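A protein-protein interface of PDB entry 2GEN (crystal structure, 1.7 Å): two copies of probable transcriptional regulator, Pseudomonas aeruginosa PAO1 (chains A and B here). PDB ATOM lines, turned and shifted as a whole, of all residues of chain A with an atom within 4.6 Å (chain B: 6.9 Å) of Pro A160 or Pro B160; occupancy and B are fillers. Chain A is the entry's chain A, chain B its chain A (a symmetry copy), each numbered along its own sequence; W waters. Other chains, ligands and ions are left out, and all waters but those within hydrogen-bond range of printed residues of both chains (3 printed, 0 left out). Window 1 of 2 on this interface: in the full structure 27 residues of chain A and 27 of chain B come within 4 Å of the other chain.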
ATOM      1  N   SER A 155      18.220 -11.532  -9.808  1.00  0.00           N
ATOM      2  CA  SER A 155      16.922 -11.724 -10.511  1.00  0.00           C
ATOM      3  C   SER A 155      15.792 -12.112  -9.596  1.00  0.00           C
ATOM      4  O   SER A 155      14.628 -11.701  -9.884  1.00  0.00           O
ATOM      5  CB  SER A 155      17.049 -12.783 -11.627  1.00  0.00           C
ATOM      6  OG  SER A 155      17.752 -12.208 -12.715  1.00  0.00           O
ATOM      7  N   VAL A 156      16.036 -12.896  -8.542  1.00  0.00           N
ATOM      8  CA  VAL A 156      14.937 -13.117  -7.583  1.00  0.00           C
ATOM      9  C   VAL A 156      14.555 -11.844  -6.866  1.00  0.00           C
ATOM     10  O   VAL A 156      13.362 -11.539  -6.779  1.00  0.00           O
ATOM     11  CB  VAL A 156      14.884 -14.451  -6.689  1.00  0.00           C
ATOM     12  CG1 VAL A 156      15.713 -15.648  -7.199  1.00  0.00           C
ATOM     13  CG2 VAL A 156      14.641 -14.296  -5.238  1.00  0.00           C
ATOM     14  N   VAL A 157      15.550 -11.055  -6.446  1.00  0.00           N
ATOM     15  CA  VAL A 157      15.192  -9.838  -5.682  1.00  0.00           C
ATOM     16  C   VAL A 157      14.431  -8.806  -6.528  1.00  0.00           C
ATOM     17  O   VAL A 157      13.379  -8.262  -6.058  1.00  0.00           O
ATOM     18  CB  VAL A 157      16.450  -9.204  -5.018  1.00  0.00           C
ATOM     19  CG1 VAL A 157      16.104  -7.793  -4.399  1.00  0.00           C
ATOM     20  CG2 VAL A 157      16.948 -10.135  -3.955  1.00  0.00           C
ATOM     21  N   ILE A 158      14.924  -8.540  -7.732  1.00  0.00           N
ATOM     22  CA  ILE A 158      14.355  -7.456  -8.583  1.00  0.00           C
ATOM     23  C   ILE A 158      13.422  -7.904  -9.707  1.00  0.00           C
ATOM     24  O   ILE A 158      12.721  -7.063 -10.321  1.00  0.00           O
ATOM     25  CB  ILE A 158      15.476  -6.485  -9.124  1.00  0.00           C
ATOM     26  CG1 ILE A 158      14.930  -5.079  -9.436  1.00  0.00           C
ATOM     27  CG2 ILE A 158      16.181  -7.058 -10.311  1.00  0.00           C
ATOM     28  CD1 ILE A 158      14.432  -4.371  -8.166  1.00  0.00           C
ATOM     29  N   GLY A 159      13.435  -9.210 -10.051  1.00  0.00           N
ATOM     30  CA  GLY A 159      12.657  -9.689 -11.206  1.00  0.00           C
ATOM     31  C   GLY A 159      11.153  -9.379 -11.059  1.00  0.00           C
ATOM     32  O   GLY A 159      10.579  -8.873 -12.010  1.00  0.00           O
ATOM     33  N   PRO A 160      10.546  -9.723  -9.913  1.00  0.00           N
ATOM     34  CA  PRO A 160       9.098  -9.383  -9.803  1.00  0.00           C
ATOM     35  C   PRO A 160       8.785  -7.894 -10.012  1.00  0.00           C
ATOM     36  O   PRO A 160       7.867  -7.546 -10.792  1.00  0.00           O
ATOM     37  CB  PRO A 160       8.728  -9.862  -8.403  1.00  0.00           C
ATOM     38  CG  PRO A 160       9.622 -11.059  -8.179  1.00  0.00           C
ATOM     39  CD  PRO A 160      10.957 -10.510  -8.733  1.00  0.00           C
ATOM     40  N   ALA A 161       9.533  -7.011  -9.348  1.00  0.00           N
ATOM     41  CA  ALA A 161       9.364  -5.586  -9.532  1.00  0.00           C
ATOM     42  C   ALA A 161       9.592  -5.162 -10.980  1.00  0.00           C
ATOM     43  O   ALA A 161       8.794  -4.421 -11.512  1.00  0.00           O
ATOM     44  CB  ALA A 161      10.316  -4.793  -8.562  1.00  0.00           C
ATOM     45  N   HIS A 162      10.676  -5.613 -11.638  1.00  0.00           N
ATOM     46  CA  HIS A 162      10.887  -5.320 -13.036  1.00  0.00           C
ATOM     47  C   HIS A 162       9.681  -5.782 -13.883  1.00  0.00           C
ATOM     48  O   HIS A 162       9.205  -5.058 -14.788  1.00  0.00           O
ATOM     49  CB  HIS A 162      12.157  -6.028 -13.547  1.00  0.00           C
ATOM     50  CG  HIS A 162      13.436  -5.328 -13.216  1.00  0.00           C
ATOM     51  ND1 HIS A 162      14.676  -5.855 -13.558  1.00  0.00           N
ATOM     52  CD2 HIS A 162      13.689  -4.155 -12.574  1.00  0.00           C
ATOM     53  CE1 HIS A 162      15.629  -5.018 -13.172  1.00  0.00           C
ATOM     54  NE2 HIS A 162      15.061  -3.980 -12.570  1.00  0.00           N
ATOM     55  N   ASP A 163       9.229  -7.001 -13.606  1.00  0.00           N
ATOM     56  CA  ASP A 163       8.165  -7.587 -14.405  1.00  0.00           C
ATOM     57  C   ASP A 163       6.844  -6.827 -14.208  1.00  0.00           C
ATOM     58  O   ASP A 163       6.187  -6.466 -15.194  1.00  0.00           O
ATOM     59  CB  ASP A 163       8.009  -9.064 -14.073  1.00  0.00           C
ATOM     60  CG  ASP A 163       7.164  -9.798 -15.090  1.00  0.00           C
ATOM     61  OD1 ASP A 163       7.672 -10.062 -16.223  1.00  0.00           O
ATOM     62  OD2 ASP A 163       6.002 -10.097 -14.758  1.00  0.00           O
ATOM     63  N   LEU A 164       6.454  -6.590 -12.962  1.00  0.00           N
ATOM     64  CA  LEU A 164       5.216  -5.833 -12.678  1.00  0.00           C
ATOM     65  C   LEU A 164       5.299  -4.411 -13.253  1.00  0.00           C
ATOM     66  O   LEU A 164       4.338  -3.929 -13.861  1.00  0.00           O
ATOM     67  CB  LEU A 164       4.937  -5.794 -11.198  1.00  0.00           C
ATOM     68  CG  LEU A 164       3.531  -5.314 -10.762  1.00  0.00           C
ATOM     69  CD1 LEU A 164       2.438  -6.114 -11.501  1.00  0.00           C
ATOM     70  CD2 LEU A 164       3.343  -5.464  -9.268  1.00  0.00           C
ATOM     71  N   LEU A 184       5.934  -6.581  -2.694  1.00  0.00           N
ATOM     72  CA  LEU A 184       7.114  -7.004  -3.491  1.00  0.00           C
ATOM     73  C   LEU A 184       8.389  -6.927  -2.617  1.00  0.00           C
ATOM     74  O   LEU A 184       9.248  -7.805  -2.678  1.00  0.00           O
ATOM     75  CB  LEU A 184       7.240  -6.184  -4.768  1.00  0.00           C
ATOM     76  CG  LEU A 184       6.160  -6.515  -5.838  1.00  0.00           C
ATOM     77  CD1 LEU A 184       6.406  -5.911  -7.182  1.00  0.00           C
ATOM     78  CD2 LEU A 184       5.962  -8.037  -5.992  1.00  0.00           C
ATOM     79  N   ILE B  92      11.597 -21.673 -18.512  1.00  0.00           N
ATOM     80  CA  ILE B  92      13.057 -21.829 -18.516  1.00  0.00           C
ATOM     81  C   ILE B  92      13.410 -22.888 -19.579  1.00  0.00           C
ATOM     82  O   ILE B  92      14.242 -22.645 -20.437  1.00  0.00           O
ATOM     83  CB  ILE B  92      13.574 -22.202 -17.115  1.00  0.00           C
ATOM     84  CG1 ILE B  92      13.431 -20.986 -16.174  1.00  0.00           C
ATOM     85  CG2 ILE B  92      15.061 -22.720 -17.218  1.00  0.00           C
ATOM     86  CD1 ILE B  92      14.238 -19.796 -16.582  1.00  0.00           C
ATOM     87  N   CYS B 152       0.155  -9.356  -9.090  1.00  0.00           N
ATOM     88  CA  CYS B 152       1.355  -9.504  -8.246  1.00  0.00           C
ATOM     89  C   CYS B 152       1.841 -10.951  -8.233  1.00  0.00           C
ATOM     90  O   CYS B 152       3.026 -11.230  -8.491  1.00  0.00           O
ATOM     91  CB  CYS B 152       1.060  -9.119  -6.816  1.00  0.00           C
ATOM     92  SG  CYS B 152       0.817  -7.396  -6.671  1.00  0.00           S
ATOM     93  N   ALA B 154       1.327 -13.209 -10.474  1.00  0.00           N
ATOM     94  CA  ALA B 154       1.898 -13.527 -11.802  1.00  0.00           C
ATOM     95  C   ALA B 154       3.368 -13.104 -11.902  1.00  0.00           C
ATOM     96  O   ALA B 154       4.238 -13.901 -12.302  1.00  0.00           O
ATOM     97  CB  ALA B 154       1.076 -12.885 -12.923  1.00  0.00           C
ATOM     98  N   SER B 155       3.629 -11.852 -11.515  1.00  0.00           N
ATOM     99  CA  SER B 155       5.005 -11.286 -11.553  1.00  0.00           C
ATOM    100  C   SER B 155       5.928 -11.878 -10.523  1.00  0.00           C
ATOM    101  O   SER B 155       7.155 -11.992 -10.823  1.00  0.00           O
ATOM    102  CB  SER B 155       4.977  -9.752 -11.377  1.00  0.00           C
ATOM    103  OG  SER B 155       4.517  -9.170 -12.585  1.00  0.00           O
ATOM    104  N   VAL B 156       5.447 -12.228  -9.327  1.00  0.00           N
ATOM    105  CA  VAL B 156       6.347 -12.953  -8.410  1.00  0.00           C
ATOM    106  C   VAL B 156       6.709 -14.319  -8.945  1.00  0.00           C
ATOM    107  O   VAL B 156       7.892 -14.671  -8.938  1.00  0.00           O
ATOM    108  CB  VAL B 156       6.136 -12.872  -6.819  1.00  0.00           C
ATOM    109  CG1 VAL B 156       5.306 -11.679  -6.300  1.00  0.00           C
ATOM    110  CG2 VAL B 156       6.145 -14.142  -6.060  1.00  0.00           C
ATOM    111  N   VAL B 157       5.728 -15.041  -9.496  1.00  0.00           N
ATOM    112  CA  VAL B 157       6.055 -16.408  -9.963  1.00  0.00           C
ATOM    113  C   VAL B 157       7.031 -16.415 -11.149  1.00  0.00           C
ATOM    114  O   VAL B 157       8.031 -17.203 -11.134  1.00  0.00           O
ATOM    115  CB  VAL B 157       4.761 -17.210 -10.293  1.00  0.00           C
ATOM    116  CG1 VAL B 157       5.117 -18.577 -11.001  1.00  0.00           C
ATOM    117  CG2 VAL B 157       4.016 -17.458  -9.018  1.00  0.00           C
ATOM    118  N   ILE B 158       6.771 -15.573 -12.143  1.00  0.00           N
ATOM    119  CA  ILE B 158       7.564 -15.592 -13.404  1.00  0.00           C
ATOM    120  C   ILE B 158       8.631 -14.506 -13.544  1.00  0.00           C
ATOM    121  O   ILE B 158       9.493 -14.579 -14.453  1.00  0.00           O
ATOM    122  CB  ILE B 158       6.635 -15.647 -14.680  1.00  0.00           C
ATOM    123  CG1 ILE B 158       7.343 -16.285 -15.890  1.00  0.00           C
ATOM    124  CG2 ILE B 158       6.093 -14.298 -15.031  1.00  0.00           C
ATOM    125  CD1 ILE B 158       7.679 -17.762 -15.634  1.00  0.00           C
ATOM    126  N   GLY B 159       8.565 -13.450 -12.705  1.00  0.00           N
ATOM    127  CA  GLY B 159       9.483 -12.309 -12.863  1.00  0.00           C
ATOM    128  C   GLY B 159      10.961 -12.738 -12.773  1.00  0.00           C
ATOM    129  O   GLY B 159      11.727 -12.332 -13.633  1.00  0.00           O
ATOM    130  N   PRO B 160      11.336 -13.497 -11.733  1.00  0.00           N
ATOM    131  CA  PRO B 160      12.769 -13.910 -11.697  1.00  0.00           C
ATOM    132  C   PRO B 160      13.237 -14.660 -12.952  1.00  0.00           C
ATOM    133  O   PRO B 160      14.299 -14.325 -13.529  1.00  0.00           O
ATOM    134  CB  PRO B 160      12.858 -14.771 -10.441  1.00  0.00           C
ATOM    135  CG  PRO B 160      11.841 -14.158  -9.506  1.00  0.00           C
ATOM    136  CD  PRO B 160      10.669 -13.932 -10.489  1.00  0.00           C
ATOM    137  N   ALA B 161      12.466 -15.655 -13.396  1.00  0.00           N
ATOM    138  CA  ALA B 161      12.783 -16.375 -14.610  1.00  0.00           C
ATOM    139  C   ALA B 161      12.837 -15.456 -15.827  1.00  0.00           C
ATOM    140  O   ALA B 161      13.773 -15.542 -16.592  1.00  0.00           O
ATOM    141  CB  ALA B 161      11.752 -17.543 -14.839  1.00  0.00           C
ATOM    142  N   HIS B 162      11.844 -14.570 -16.031  1.00  0.00           N
ATOM    143  CA  HIS B 162      11.896 -13.613 -17.111  1.00  0.00           C
ATOM    144  C   HIS B 162      13.183 -12.763 -17.032  1.00  0.00           C
ATOM    145  O   HIS B 162      13.863 -12.516 -18.055  1.00  0.00           O
ATOM    146  CB  HIS B 162      10.674 -12.675 -17.056  1.00  0.00           C
ATOM    147  CG  HIS B 162       9.422 -13.250 -17.636  1.00  0.00           C
ATOM    148  ND1 HIS B 162       8.216 -12.557 -17.622  1.00  0.00           N
ATOM    149  CD2 HIS B 162       9.164 -14.442 -18.240  1.00  0.00           C
ATOM    150  CE1 HIS B 162       7.286 -13.285 -18.225  1.00  0.00           C
ATOM    151  NE2 HIS B 162       7.832 -14.434 -18.607  1.00  0.00           N
ATOM    152  N   ASP B 163      13.478 -12.293 -15.825  1.00  0.00           N
ATOM    153  CA  ASP B 163      14.608 -11.397 -15.643  1.00  0.00           C
ATOM    154  C   ASP B 163      15.937 -12.119 -15.913  1.00  0.00           C
ATOM    155  O   ASP B 163      16.777 -11.604 -16.663  1.00  0.00           O
ATOM    156  CB  ASP B 163      14.581 -10.790 -14.247  1.00  0.00           C
ATOM    157  CG  ASP B 163      15.519  -9.612 -14.111  1.00  0.00           C
ATOM    158  OD1 ASP B 163      15.187  -8.508 -14.644  1.00  0.00           O
ATOM    159  OD2 ASP B 163      16.579  -9.797 -13.486  1.00  0.00           O
ATOM    160  N   LEU B 164      16.130 -13.287 -15.313  1.00  0.00           N
ATOM    161  CA  LEU B 164      17.363 -14.070 -15.544  1.00  0.00           C
ATOM    162  C   LEU B 164      17.498 -14.455 -17.026  1.00  0.00           C
ATOM    163  O   LEU B 164      18.584 -14.341 -17.602  1.00  0.00           O
ATOM    164  CB  LEU B 164      17.393 -15.297 -14.670  1.00  0.00           C
ATOM    165  CG  LEU B 164      18.742 -16.051 -14.564  1.00  0.00           C
ATOM    166  CD1 LEU B 164      19.871 -15.075 -14.173  1.00  0.00           C
ATOM    167  CD2 LEU B 164      18.663 -17.167 -13.546  1.00  0.00           C
ATOM    168  N   ALA B 165      16.397 -14.881 -17.651  1.00  0.00           N
ATOM    169  CA  ALA B 165      16.432 -15.235 -19.067  1.00  0.00           C
ATOM    170  C   ALA B 165      16.891 -14.063 -19.933  1.00  0.00           C
ATOM    171  O   ALA B 165      17.763 -14.222 -20.793  1.00  0.00           O
ATOM    172  CB  ALA B 165      15.073 -15.719 -19.526  1.00  0.00           C
ATOM    173  N   ARG B 166      16.310 -12.887 -19.686  1.00  0.00           N
ATOM    174  CA  ARG B 166      16.718 -11.652 -20.380  1.00  0.00           C
ATOM    175  C   ARG B 166      18.252 -11.409 -20.258  1.00  0.00           C
ATOM    176  O   ARG B 166      18.953 -11.239 -21.276  1.00  0.00           O
ATOM    177  CB  ARG B 166      15.888 -10.475 -19.826  1.00  0.00           C
ATOM    178  CG  ARG B 166      15.826  -9.255 -20.701  1.00  0.00           C
ATOM    179  CD  ARG B 166      14.819  -8.175 -20.162  1.00  0.00           C
ATOM    180  NE  ARG B 166      13.406  -8.353 -20.516  1.00  0.00           N
ATOM    181  CZ  ARG B 166      12.845  -7.979 -21.675  1.00  0.00           C
ATOM    182  NH1 ARG B 166      13.576  -7.439 -22.645  1.00  0.00           N
ATOM    183  NH2 ARG B 166      11.546  -8.180 -21.880  1.00  0.00           N
ATOM    184  N   LEU B 177      21.620 -20.666 -17.580  1.00  0.00           N
ATOM    185  CA  LEU B 177      20.162 -20.637 -17.285  1.00  0.00           C
ATOM    186  C   LEU B 177      19.592 -21.983 -16.822  1.00  0.00           C
ATOM    187  O   LEU B 177      18.869 -21.992 -15.817  1.00  0.00           O
ATOM    188  CB  LEU B 177      19.333 -20.065 -18.452  1.00  0.00           C
ATOM    189  CG  LEU B 177      17.845 -19.793 -18.148  1.00  0.00           C
ATOM    190  CD1 LEU B 177      17.655 -18.779 -17.014  1.00  0.00           C
ATOM    191  CD2 LEU B 177      17.091 -19.337 -19.396  1.00  0.00           C
ATOM    192  N   LEU B 184      14.923 -21.518  -9.274  1.00  0.00           N
ATOM    193  CA  LEU B 184      13.861 -20.531  -9.598  1.00  0.00           C
ATOM    194  C   LEU B 184      12.469 -21.166  -9.365  1.00  0.00           C
ATOM    195  O   LEU B 184      11.562 -20.519  -8.844  1.00  0.00           O
ATOM    196  CB  LEU B 184      14.021 -19.993 -11.013  1.00  0.00           C
ATOM    197  CG  LEU B 184      15.233 -19.034 -11.189  1.00  0.00           C
ATOM    198  CD1 LEU B 184      15.267 -18.303 -12.492  1.00  0.00           C
ATOM    199  CD2 LEU B 184      15.325 -18.018 -10.032  1.00  0.00           C
ATOM    200  N   VAL B 187      12.045 -21.277  -5.502  1.00  0.00           N
ATOM    201  CA  VAL B 187      11.814 -19.958  -4.981  1.00  0.00           C
ATOM    202  C   VAL B 187      10.416 -19.468  -5.332  1.00  0.00           C
ATOM    203  O   VAL B 187       9.776 -18.853  -4.498  1.00  0.00           O
ATOM    204  CB  VAL B 187      12.793 -18.974  -5.503  1.00  0.00           C
ATOM    205  CG1 VAL B 187      12.326 -17.544  -5.165  1.00  0.00           C
ATOM    206  CG2 VAL B 187      14.245 -19.299  -4.922  1.00  0.00           C
ATOM    207  N   ALA B 188       9.942 -19.760  -6.539  1.00  0.00           N
ATOM    208  CA  ALA B 188       8.575 -19.299  -6.939  1.00  0.00           C
ATOM    209  C   ALA B 188       7.571 -19.897  -5.929  1.00  0.00           C
ATOM    210  O   ALA B 188       6.687 -19.179  -5.407  1.00  0.00           O
ATOM    211  CB  ALA B 188       8.259 -19.775  -8.370  1.00  0.00           C
ATOM    212  N   SER B 191       7.872 -18.406  -2.513  1.00  0.00           N
ATOM    213  CA  SER B 191       7.509 -17.007  -2.503  1.00  0.00           C
ATOM    214  C   SER B 191       6.006 -16.840  -2.414  1.00  0.00           C
ATOM    215  O   SER B 191       5.550 -15.886  -1.809  1.00  0.00           O
ATOM    216  CB  SER B 191       8.010 -16.272  -3.730  1.00  0.00           C
ATOM    217  OG  SER B 191       9.425 -16.264  -3.720  1.00  0.00           O
HETATM  218  O   HOH W   1      11.351  -9.657 -14.696  1.00  0.00           O
HETATM  219  O   HOH W   2       5.169 -11.190 -17.328  1.00  0.00           O
HETATM  220  O   HOH W   3      17.736  -7.165 -13.966  1.00  0.00           O
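OG of Ser B191 is in hydrogen-bond range of O of Val B187 (2.7 Å).
Among the printed residues, pairs that only touch across the chains: Ser A155 with Pro B160 (3.4 Å), Val A156 with Pro B160 (3.8 Å), Val A156 with Leu B184 (3.7 Å), Val A156 with Val B187 (3.99 Å), Gly A159 with Gly B159 (3.7 Å), Gly A159 with Asp B163 (3.8 Å), Pro A160 with Ser B155 (3.4 Å), Pro A160 with Val B156 (3.8 Å), Pro A160 with Pro B160 (3.8 Å), Asp A163 with Gly B159 (3.8 Å) and Leu A184 with Val B156 (3.7 Å).
Water W1 lies within hydrogen-bond range of O of Gly A159 and O of Gly B159.
Water W2 lies within hydrogen-bond range of OD2 of Asp A163 (2.9 Å) and ND1 of His B162 (3.4 Å).
Water W3 lies within hydrogen-bond range of OD2 of Asp B163 (2.9 Å) and ND1 of His A162 (3.4 Å).
Of the printed residues of chain B, Val A156 touches Pro B160 (3.8 Å), Leu B184 (3.7 Å) and Val B187 (3.99 Å).
Of the printed residues of chain B, Asp A163 touches Ser B155 (2.8 Å), Gly B159 (3.8 Å) and His B162 (2.9 Å).
Of the printed residues of chain A, Val B156 touches Pro A160 (3.8 Å) and Leu A184 (3.7 Å).
Of the printed residues of chain A, Pro B160 touches Ser A155, Val A156 and Pro A160.
Of the printed residues of chain A, His B162 touches Asp A163 (2.9 Å).
The backbone NH of Leu A164 sits at hydrogen-bond distance from the side-chain hydroxyl of Ser B155 (3.2 Å).
A ring nitrogen (ND1) of His B162 sits at hydrogen-bond distance from the side-chain carboxylate (OD1) of Asp A163 (2.9 Å).
OG of Ser A155 sits at hydrogen-bond distance from OD2 of Asp B163.
The side-chain carboxylate of Asp B163 lies within hydrogen-bond range of a ring nitrogen (ND1) of His A162 (2.9 Å).
The side-chain hydroxyl of Ser B155 is in hydrogen-bond range of the side-chain carboxylate of Asp A163 (2.8 Å).
N of Leu B164 sits at hydrogen-bond distance from OG of Ser A155, 3.2 Å away.
Of the 20 printed residues of chain B, 9 touch a printed residue of chain A.
Printed residues of chain B that touch a printed residue of chain A: Ser B155, Val B156, Gly B159, Pro B160, His B162, Asp B163, Leu B164, Leu B184 and Val B187.
Of the 11 printed residues of chain A, 8 touch a printed residue of chain B.
Hydrophobic or aromatic side chains of chain A within 4 Å of the printed part of chain B: Val A156, Pro A160, His A162, Leu A164 and Leu A184.
Among the printed residues, 17 pairs touch across the chains.
Among the printed residues, no Asp or Glu carboxylate lies within 4 Å of a Lys or Arg side-chain nitrogen of the other chain.
Ser A155 touches Pro B160, and with the chains exchanged Pro A160 touches Ser B155.
Ser A155 touches Asp B163, and with the chains exchanged Asp A163 touches Ser B155.
Gly A159 touches Asp B163, and with the chains exchanged Asp A163 touches Gly B159.
Pro B160 touches its own counterpart, Pro A160.
Of the 17 pairs that touch across the chains among the printed residues, 16 have their exchanged pair printed and touching as well.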
